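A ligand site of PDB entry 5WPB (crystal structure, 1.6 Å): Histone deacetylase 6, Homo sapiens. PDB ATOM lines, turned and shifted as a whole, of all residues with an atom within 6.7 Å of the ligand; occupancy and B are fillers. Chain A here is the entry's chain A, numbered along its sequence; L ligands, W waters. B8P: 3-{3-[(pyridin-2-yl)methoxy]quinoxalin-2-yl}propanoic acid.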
ATOM      1  N   GLU A  35     -29.427   1.589  11.870  1.00  0.00           N
ATOM      2  CA  GLU A  35     -28.399   0.798  12.560  1.00  0.00           C
ATOM      3  C   GLU A  35     -27.307   1.644  13.192  1.00  0.00           C
ATOM      4  O   GLU A  35     -26.126   1.354  13.064  1.00  0.00           O
ATOM      5  CB  GLU A  35     -27.805  -0.306  11.640  1.00  0.00           C
ATOM      6  CG  GLU A  35     -27.101  -1.453  12.388  1.00  0.00           C
ATOM      7  CD  GLU A  35     -26.623  -2.612  11.493  1.00  0.00           C
ATOM      8  OE1 GLU A  35     -27.446  -3.552  11.349  1.00  0.00           O
ATOM      9  OE2 GLU A  35     -25.439  -2.623  10.973  1.00  0.00           O
ATOM     10  N   ASN A  36     -27.709   2.708  13.872  1.00  0.00           N
ATOM     11  CA  ASN A  36     -26.739   3.532  14.555  1.00  0.00           C
ATOM     12  C   ASN A  36     -26.327   2.990  15.918  1.00  0.00           C
ATOM     13  O   ASN A  36     -27.064   2.263  16.609  1.00  0.00           O
ATOM     14  CB  ASN A  36     -27.222   4.977  14.640  1.00  0.00           C
ATOM     15  CG  ASN A  36     -27.183   5.643  13.275  1.00  0.00           C
ATOM     16  OD1 ASN A  36     -26.141   5.681  12.647  1.00  0.00           O
ATOM     17  ND2 ASN A  36     -28.339   6.141  12.815  1.00  0.00           N
ATOM     18  N   TRP A  37     -25.119   3.377  16.272  1.00  0.00           N
ATOM     19  CA  TRP A  37     -24.462   3.031  17.542  1.00  0.00           C
ATOM     20  C   TRP A  37     -23.954   4.309  18.151  1.00  0.00           C
ATOM     21  O   TRP A  37     -23.661   5.260  17.421  1.00  0.00           O
ATOM     22  CB  TRP A  37     -23.274   2.112  17.271  1.00  0.00           C
ATOM     23  CG  TRP A  37     -23.620   0.771  16.715  1.00  0.00           C
ATOM     24  CD1 TRP A  37     -24.005   0.474  15.418  1.00  0.00           C
ATOM     25  CD2 TRP A  37     -23.601  -0.474  17.413  1.00  0.00           C
ATOM     26  NE1 TRP A  37     -24.232  -0.858  15.287  1.00  0.00           N
ATOM     27  CE2 TRP A  37     -23.976  -1.473  16.486  1.00  0.00           C
ATOM     28  CE3 TRP A  37     -23.329  -0.843  18.732  1.00  0.00           C
ATOM     29  CZ2 TRP A  37     -24.093  -2.803  16.841  1.00  0.00           C
ATOM     30  CZ3 TRP A  37     -23.394  -2.185  19.076  1.00  0.00           C
ATOM     31  CH2 TRP A  37     -23.775  -3.155  18.126  1.00  0.00           C
ATOM     32  N   CYS A  47     -22.986   4.836  12.105  1.00  0.00           N
ATOM     33  CA  CYS A  47     -23.739   3.685  11.641  1.00  0.00           C
ATOM     34  C   CYS A  47     -22.979   2.357  11.677  1.00  0.00           C
ATOM     35  O   CYS A  47     -21.743   2.292  11.677  1.00  0.00           O
ATOM     36  CB  CYS A  47     -24.315   3.971  10.245  1.00  0.00           C
ATOM     37  SG  CYS A  47     -23.097   4.074   8.901  1.00  0.00           S
ATOM     38  N   GLY A  48     -23.780   1.304  11.686  1.00  0.00           N
ATOM     39  CA  GLY A  48     -23.295  -0.061  11.780  1.00  0.00           C
ATOM     40  C   GLY A  48     -22.696  -0.613  10.503  1.00  0.00           C
ATOM     41  O   GLY A  48     -22.819  -0.057   9.412  1.00  0.00           O
ATOM     42  N   ARG A  49     -22.098  -1.798  10.676  1.00  0.00           N
ATOM     43  CA  ARG A  49     -21.338  -2.396   9.582  1.00  0.00           C
ATOM     44  C   ARG A  49     -22.182  -2.831   8.398  1.00  0.00           C
ATOM     45  O   ARG A  49     -21.695  -2.800   7.280  1.00  0.00           O
ATOM     46  CB  ARG A  49     -20.398  -3.496  10.082  1.00  0.00           C
ATOM     47  CG  ARG A  49     -21.006  -4.815  10.465  1.00  0.00           C
ATOM     48  CD  ARG A  49     -20.586  -5.973   9.550  1.00  0.00           C
ATOM     49  N   TYR A  50     -23.470  -3.075   8.591  1.00  0.00           N
ATOM     50  CA  TYR A  50     -24.356  -3.433   7.487  1.00  0.00           C
ATOM     51  C   TYR A  50     -24.915  -2.232   6.730  1.00  0.00           C
ATOM     52  O   TYR A  50     -25.551  -2.396   5.677  1.00  0.00           O
ATOM     53  CB  TYR A  50     -25.491  -4.377   7.982  1.00  0.00           C
ATOM     54  CG  TYR A  50     -24.958  -5.734   8.449  1.00  0.00           C
ATOM     55  CD1 TYR A  50     -24.288  -6.559   7.546  1.00  0.00           C
ATOM     56  CD2 TYR A  50     -25.072  -6.160   9.756  1.00  0.00           C
ATOM     57  CE1 TYR A  50     -23.770  -7.799   7.942  1.00  0.00           C
ATOM     58  CE2 TYR A  50     -24.565  -7.389  10.160  1.00  0.00           C
ATOM     59  CZ  TYR A  50     -23.934  -8.243   9.242  1.00  0.00           C
ATOM     60  OH  TYR A  50     -23.423  -9.481   9.678  1.00  0.00           O
ATOM     61  N   GLY A  53     -20.742   1.442   7.773  1.00  0.00           N
ATOM     62  CA  GLY A  53     -19.580   1.103   8.580  1.00  0.00           C
ATOM     63  C   GLY A  53     -18.874   2.247   9.260  1.00  0.00           C
ATOM     64  O   GLY A  53     -17.677   2.189   9.548  1.00  0.00           O
ATOM     65  N   HIS A  54     -19.597   3.322   9.560  1.00  0.00           N
ATOM     66  CA  HIS A  54     -18.940   4.501  10.118  1.00  0.00           C
ATOM     67  C   HIS A  54     -18.524   4.314  11.572  1.00  0.00           C
ATOM     68  O   HIS A  54     -17.557   4.914  12.004  1.00  0.00           O
ATOM     69  CB  HIS A  54     -19.757   5.770   9.873  1.00  0.00           C
ATOM     70  CG  HIS A  54     -19.745   6.152   8.439  1.00  0.00           C
ATOM     71  ND1 HIS A  54     -20.890   6.333   7.685  1.00  0.00           N
ATOM     72  CD2 HIS A  54     -18.693   6.288   7.593  1.00  0.00           C
ATOM     73  CE1 HIS A  54     -20.529   6.603   6.450  1.00  0.00           C
ATOM     74  NE2 HIS A  54     -19.206   6.560   6.362  1.00  0.00           N
ATOM     75  N   MET A  55     -19.228   3.470  12.347  1.00  0.00           N
ATOM     76  CA  MET A  55     -18.737   3.246  13.714  1.00  0.00           C
ATOM     77  C   MET A  55     -17.446   2.397  13.690  1.00  0.00           C
ATOM     78  O   MET A  55     -16.550   2.637  14.478  1.00  0.00           O
ATOM     79  CB  MET A  55     -19.805   2.674  14.645  1.00  0.00           C
ATOM     80  CG  MET A  55     -19.327   2.617  16.111  1.00  0.00           C
ATOM     81  SD  MET A  55     -18.948   4.252  16.767  1.00  0.00           S
ATOM     82  CE  MET A  55     -20.573   4.752  17.325  1.00  0.00           C
ATOM     83  N   LEU A  56     -17.368   1.432  12.786  1.00  0.00           N
ATOM     84  CA  LEU A  56     -16.143   0.678  12.623  1.00  0.00           C
ATOM     85  C   LEU A  56     -15.008   1.628  12.250  1.00  0.00           C
ATOM     86  O   LEU A  56     -13.895   1.487  12.782  1.00  0.00           O
ATOM     87  CB  LEU A  56     -16.331  -0.434  11.592  1.00  0.00           C
ATOM     88  CG  LEU A  56     -15.072  -1.265  11.337  1.00  0.00           C
ATOM     89  CD1 LEU A  56     -14.641  -2.036  12.555  1.00  0.00           C
ATOM     90  CD2 LEU A  56     -15.387  -2.209  10.183  1.00  0.00           C
ATOM     91  N   GLN A  57     -15.277   2.592  11.363  1.00  0.00           N
ATOM     92  CA  GLN A  57     -14.293   3.598  10.992  1.00  0.00           C
ATOM     93  C   GLN A  57     -13.892   4.422  12.219  1.00  0.00           C
ATOM     94  O   GLN A  57     -12.703   4.712  12.433  1.00  0.00           O
ATOM     95  CB  GLN A  57     -14.848   4.489   9.868  1.00  0.00           C
ATOM     96  CG  GLN A  57     -13.878   5.518   9.340  1.00  0.00           C
ATOM     97  CD  GLN A  57     -14.389   6.217   8.053  1.00  0.00           C
ATOM     98  OE1 GLN A  57     -15.317   5.735   7.406  1.00  0.00           O
ATOM     99  NE2 GLN A  57     -13.755   7.336   7.666  1.00  0.00           N
ATOM    100  N   VAL A  67     -19.189   0.189  22.043  1.00  0.00           N
ATOM    101  CA  VAL A  67     -20.279   0.956  21.415  1.00  0.00           C
ATOM    102  C   VAL A  67     -21.602   0.301  21.749  1.00  0.00           C
ATOM    103  O   VAL A  67     -21.664  -0.900  21.923  1.00  0.00           O
ATOM    104  CB  VAL A  67     -20.043   1.095  19.882  1.00  0.00           C
ATOM    105  CG1 VAL A  67     -18.761   1.856  19.627  1.00  0.00           C
ATOM    106  CG2 VAL A  67     -19.962  -0.259  19.196  1.00  0.00           C
ATOM    107  N   SER A  69     -25.687  -0.234  20.804  1.00  0.00           N
ATOM    108  CA  SER A  69     -26.632  -0.251  19.680  1.00  0.00           C
ATOM    109  C   SER A  69     -27.931   0.456  20.027  1.00  0.00           C
ATOM    110  O   SER A  69     -28.599   0.165  21.039  1.00  0.00           O
ATOM    111  CB  SER A  69     -27.011  -1.691  19.297  1.00  0.00           C
ATOM    112  OG  SER A  69     -28.029  -1.638  18.318  1.00  0.00           O
ATOM    113  N   TYR A  70     -28.324   1.375  19.152  1.00  0.00           N
ATOM    114  CA  TYR A  70     -29.644   1.969  19.248  1.00  0.00           C
ATOM    115  C   TYR A  70     -30.773   1.119  18.712  1.00  0.00           C
ATOM    116  O   TYR A  70     -31.941   1.536  18.783  1.00  0.00           O
ATOM    117  CB  TYR A  70     -29.599   3.335  18.604  1.00  0.00           C
ATOM    118  CG  TYR A  70     -28.895   4.436  19.408  1.00  0.00           C
ATOM    119  CD1 TYR A  70     -28.712   4.346  20.817  1.00  0.00           C
ATOM    120  CD2 TYR A  70     -28.461   5.588  18.772  1.00  0.00           C
ATOM    121  CE1 TYR A  70     -28.156   5.387  21.528  1.00  0.00           C
ATOM    122  CE2 TYR A  70     -27.895   6.629  19.486  1.00  0.00           C
ATOM    123  CZ  TYR A  70     -27.750   6.529  20.878  1.00  0.00           C
ATOM    124  OH  TYR A  70     -27.246   7.535  21.644  1.00  0.00           O
ATOM    125  N   ILE A  71     -30.449  -0.054  18.178  1.00  0.00           N
ATOM    126  CA  ILE A  71     -31.437  -1.071  17.798  1.00  0.00           C
ATOM    127  C   ILE A  71     -31.867  -1.818  19.070  1.00  0.00           C
ATOM    128  O   ILE A  71     -33.018  -1.742  19.521  1.00  0.00           O
ATOM    129  CB  ILE A  71     -30.865  -2.042  16.734  1.00  0.00           C
ATOM    130  CG1 ILE A  71     -30.444  -1.295  15.460  1.00  0.00           C
ATOM    131  CG2 ILE A  71     -31.865  -3.145  16.418  1.00  0.00           C
ATOM    132  CD1 ILE A  71     -31.576  -0.687  14.641  1.00  0.00           C
ATOM    133  N   ASP A  72     -30.924  -2.531  19.670  1.00  0.00           N
ATOM    134  CA  ASP A  72     -31.250  -3.515  20.711  1.00  0.00           C
ATOM    135  C   ASP A  72     -30.561  -3.296  22.054  1.00  0.00           C
ATOM    136  O   ASP A  72     -30.724  -4.104  22.939  1.00  0.00           O
ATOM    137  CB  ASP A  72     -31.008  -4.945  20.198  1.00  0.00           C
ATOM    138  CG  ASP A  72     -29.561  -5.296  20.048  1.00  0.00           C
ATOM    139  OD1 ASP A  72     -28.712  -4.446  20.202  1.00  0.00           O
ATOM    140  OD2 ASP A  72     -29.261  -6.491  19.826  1.00  0.00           O
ATOM    141  N   LEU A  73     -29.814  -2.193  22.195  1.00  0.00           N
ATOM    142  CA  LEU A  73     -29.136  -1.839  23.447  1.00  0.00           C
ATOM    143  C   LEU A  73     -28.082  -2.868  23.830  1.00  0.00           C
ATOM    144  O   LEU A  73     -27.705  -2.939  24.996  1.00  0.00           O
ATOM    145  CB  LEU A  73     -30.150  -1.629  24.603  1.00  0.00           C
ATOM    146  CG  LEU A  73     -31.336  -0.702  24.265  1.00  0.00           C
ATOM    147  CD1 LEU A  73     -32.209  -0.474  25.485  1.00  0.00           C
ATOM    148  CD2 LEU A  73     -30.852   0.613  23.718  1.00  0.00           C
ATOM    149  N   SER A  74     -27.552  -3.602  22.867  1.00  0.00           N
ATOM    150  CA  SER A  74     -26.380  -4.432  23.126  1.00  0.00           C
ATOM    151  C   SER A  74     -25.131  -3.571  23.021  1.00  0.00           C
ATOM    152  O   SER A  74     -25.131  -2.545  22.350  1.00  0.00           O
ATOM    153  CB  SER A  74     -26.265  -5.571  22.158  1.00  0.00           C
ATOM    154  OG  SER A  74     -26.169  -5.125  20.837  1.00  0.00           O
ATOM    155  N   TRP A  76     -21.019  -3.713  22.041  1.00  0.00           N
ATOM    156  CA  TRP A  76     -20.016  -4.442  21.280  1.00  0.00           C
ATOM    157  C   TRP A  76     -18.646  -3.836  21.556  1.00  0.00           C
ATOM    158  O   TRP A  76     -18.480  -2.609  21.551  1.00  0.00           O
ATOM    159  CB  TRP A  76     -20.301  -4.304  19.770  1.00  0.00           C
ATOM    160  CG  TRP A  76     -19.311  -4.971  18.860  1.00  0.00           C
ATOM    161  CD1 TRP A  76     -18.311  -4.364  18.150  1.00  0.00           C
ATOM    162  CD2 TRP A  76     -19.245  -6.363  18.550  1.00  0.00           C
ATOM    163  NE1 TRP A  76     -17.614  -5.310  17.431  1.00  0.00           N
ATOM    164  CE2 TRP A  76     -18.179  -6.542  17.634  1.00  0.00           C
ATOM    165  CE3 TRP A  76     -19.994  -7.476  18.957  1.00  0.00           C
ATOM    166  CZ2 TRP A  76     -17.851  -7.804  17.116  1.00  0.00           C
ATOM    167  CZ3 TRP A  76     -19.665  -8.719  18.438  1.00  0.00           C
ATOM    168  CH2 TRP A  76     -18.590  -8.857  17.532  1.00  0.00           C
ATOM    169  N   TYR A  78     -14.938  -3.717  19.952  1.00  0.00           N
ATOM    170  CA  TYR A  78     -14.194  -3.942  18.710  1.00  0.00           C
ATOM    171  C   TYR A  78     -12.859  -4.630  18.928  1.00  0.00           C
ATOM    172  O   TYR A  78     -12.344  -5.212  17.963  1.00  0.00           O
ATOM    173  CB  TYR A  78     -13.936  -2.627  18.004  1.00  0.00           C
ATOM    174  CG  TYR A  78     -15.179  -2.025  17.360  1.00  0.00           C
ATOM    175  CD1 TYR A  78     -15.701  -2.532  16.175  1.00  0.00           C
ATOM    176  CD2 TYR A  78     -15.836  -0.948  17.925  1.00  0.00           C
ATOM    177  CE1 TYR A  78     -16.833  -1.972  15.583  1.00  0.00           C
ATOM    178  CE2 TYR A  78     -16.968  -0.399  17.334  1.00  0.00           C
ATOM    179  CZ  TYR A  78     -17.465  -0.914  16.184  1.00  0.00           C
ATOM    180  OH  TYR A  78     -18.569  -0.354  15.607  1.00  0.00           O
ATOM    181  N   TYR A  83     -19.933  -9.119  22.136  1.00  0.00           N
ATOM    182  CA  TYR A  83     -20.838  -8.389  22.975  1.00  0.00           C
ATOM    183  C   TYR A  83     -20.462  -8.544  24.430  1.00  0.00           C
ATOM    184  O   TYR A  83     -19.934  -9.592  24.857  1.00  0.00           O
ATOM    185  CB  TYR A  83     -22.297  -8.828  22.774  1.00  0.00           C
ATOM    186  CG  TYR A  83     -22.790  -8.566  21.364  1.00  0.00           C
ATOM    187  CD1 TYR A  83     -23.229  -7.288  20.989  1.00  0.00           C
ATOM    188  CD2 TYR A  83     -22.819  -9.578  20.425  1.00  0.00           C
ATOM    189  CE1 TYR A  83     -23.703  -7.081  19.697  1.00  0.00           C
ATOM    190  CE2 TYR A  83     -23.259  -9.363  19.118  1.00  0.00           C
ATOM    191  CZ  TYR A  83     -23.706  -8.112  18.783  1.00  0.00           C
ATOM    192  OH  TYR A  83     -24.140  -7.947  17.491  1.00  0.00           O
HETATM  193  C4  B8P L   1     -21.123  -7.413  13.113  1.00  0.00           C
HETATM  194  C2  B8P L   1     -21.125  -5.353  14.867  1.00  0.00           C
HETATM  195  N1  B8P L   1     -19.959  -5.758  14.460  1.00  0.00           N
HETATM  196  C6  B8P L   1     -19.814  -8.945  11.802  1.00  0.00           C
HETATM  197  C5  B8P L   1     -21.030  -8.507  12.220  1.00  0.00           C
HETATM  198  O2  B8P L   1     -19.767  -1.530  13.646  1.00  0.00           O
HETATM  199  C16 B8P L   1     -20.543  -2.344  14.021  1.00  0.00           C
HETATM  200  O1  B8P L   1     -21.587  -2.685  13.306  1.00  0.00           O
HETATM  201  C   B8P L   1     -20.293  -3.022  15.355  1.00  0.00           C
HETATM  202  C1  B8P L   1     -21.253  -4.138  15.747  1.00  0.00           C
HETATM  203  C9  B8P L   1     -19.935  -6.790  13.561  1.00  0.00           C
HETATM  204  C8  B8P L   1     -18.688  -7.262  13.080  1.00  0.00           C
HETATM  205  C7  B8P L   1     -18.639  -8.303  12.216  1.00  0.00           C
HETATM  206  N   B8P L   1     -22.355  -7.014  13.550  1.00  0.00           N
HETATM  207  C3  B8P L   1     -22.341  -6.026  14.397  1.00  0.00           C
HETATM  208  O   B8P L   1     -23.487  -5.584  14.938  1.00  0.00           O
HETATM  209  C10 B8P L   1     -24.717  -6.205  14.493  1.00  0.00           C
HETATM  210  C11 B8P L   1     -25.829  -5.648  15.327  1.00  0.00           C
HETATM  211  N2  B8P L   1     -25.786  -5.990  16.625  1.00  0.00           N
HETATM  212  C15 B8P L   1     -26.712  -5.452  17.432  1.00  0.00           C
HETATM  213  C14 B8P L   1     -27.701  -4.598  16.999  1.00  0.00           C
HETATM  214  C13 B8P L   1     -27.718  -4.258  15.675  1.00  0.00           C
HETATM  215  C12 B8P L   1     -26.773  -4.791  14.810  1.00  0.00           C
HETATM  216  O   HOH W   1     -17.753  -4.220  13.257  1.00  0.00           O
HETATM  217  O   HOH W   2     -24.228  -3.003  13.447  1.00  0.00           O
HETATM  218  O   HOH W   3     -19.749   0.297  11.689  1.00  0.00           O
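O1 of the ligand is in hydrogen-bond range of N of Arg 49 (2.8 Å). OH of Tyr 83 is in hydrogen-bond range of N2 of the ligand, at 2.7 Å. An oxygen (O2) of the ligand sits at hydrogen-bond distance from the side-chain hydroxyl (OH) of Tyr 78 (2.6 Å).
The backbone NH (N) of Arg 49 sits at hydrogen-bond distance from the side-chain carboxylate (OE2) of Glu 35 (3.5 Å). The backbone NH of Tyr 50 lies within hydrogen-bond range of the side-chain carboxylate of Glu 35, at 3.1 Å. The side-chain hydroxyl of Ser 69 lies within hydrogen-bond range of the backbone NH of Ile 71 (2.9 Å). The backbone NH of Trp 76 is in hydrogen-bond range of the backbone carbonyl oxygen of Val 67, 2.9 Å away. The backbone carbonyl oxygen (O) of Glu 35 lies within hydrogen-bond range of the backbone NH (N) of Gly 48, 2.7 Å away. OG of Ser 69 sits at hydrogen-bond distance from N of Asp 72 (3.3 Å). OD1 of Asp 72 lies within hydrogen-bond range of OG of Ser 74, 2.7 Å away. The backbone NH (N) of Gly 53 is in hydrogen-bond range of the backbone carbonyl oxygen (O) of Gly 48 (3.0 Å).
Water W2 lies within hydrogen-bond range of an oxygen (O1) of the ligand, the side-chain carboxylate (OE2) of Glu 35 and the indole nitrogen (NE1) of Trp 37.
Residues that only touch the ligand: Glu 35 (3.7 Å), Trp 37 (3.3 Å), Gly 48 (3.5 Å), Tyr 50 (3.6 Å), Leu 56 (3.9 Å), Ser 69 (3.3 Å), Ile 71 (3.99 Å), Asp 72 (3.4 Å), Ser 74 (3.5 Å) and Trp 76 (3.7 Å). Hydrophobic or aromatic side chains within 4 Å of the ligand: Trp 37, Ile 71, Trp 76, Tyr 78 and Tyr 83. The nearest printed residue that does not touch the ligand is Met 55 (4.3 Å).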
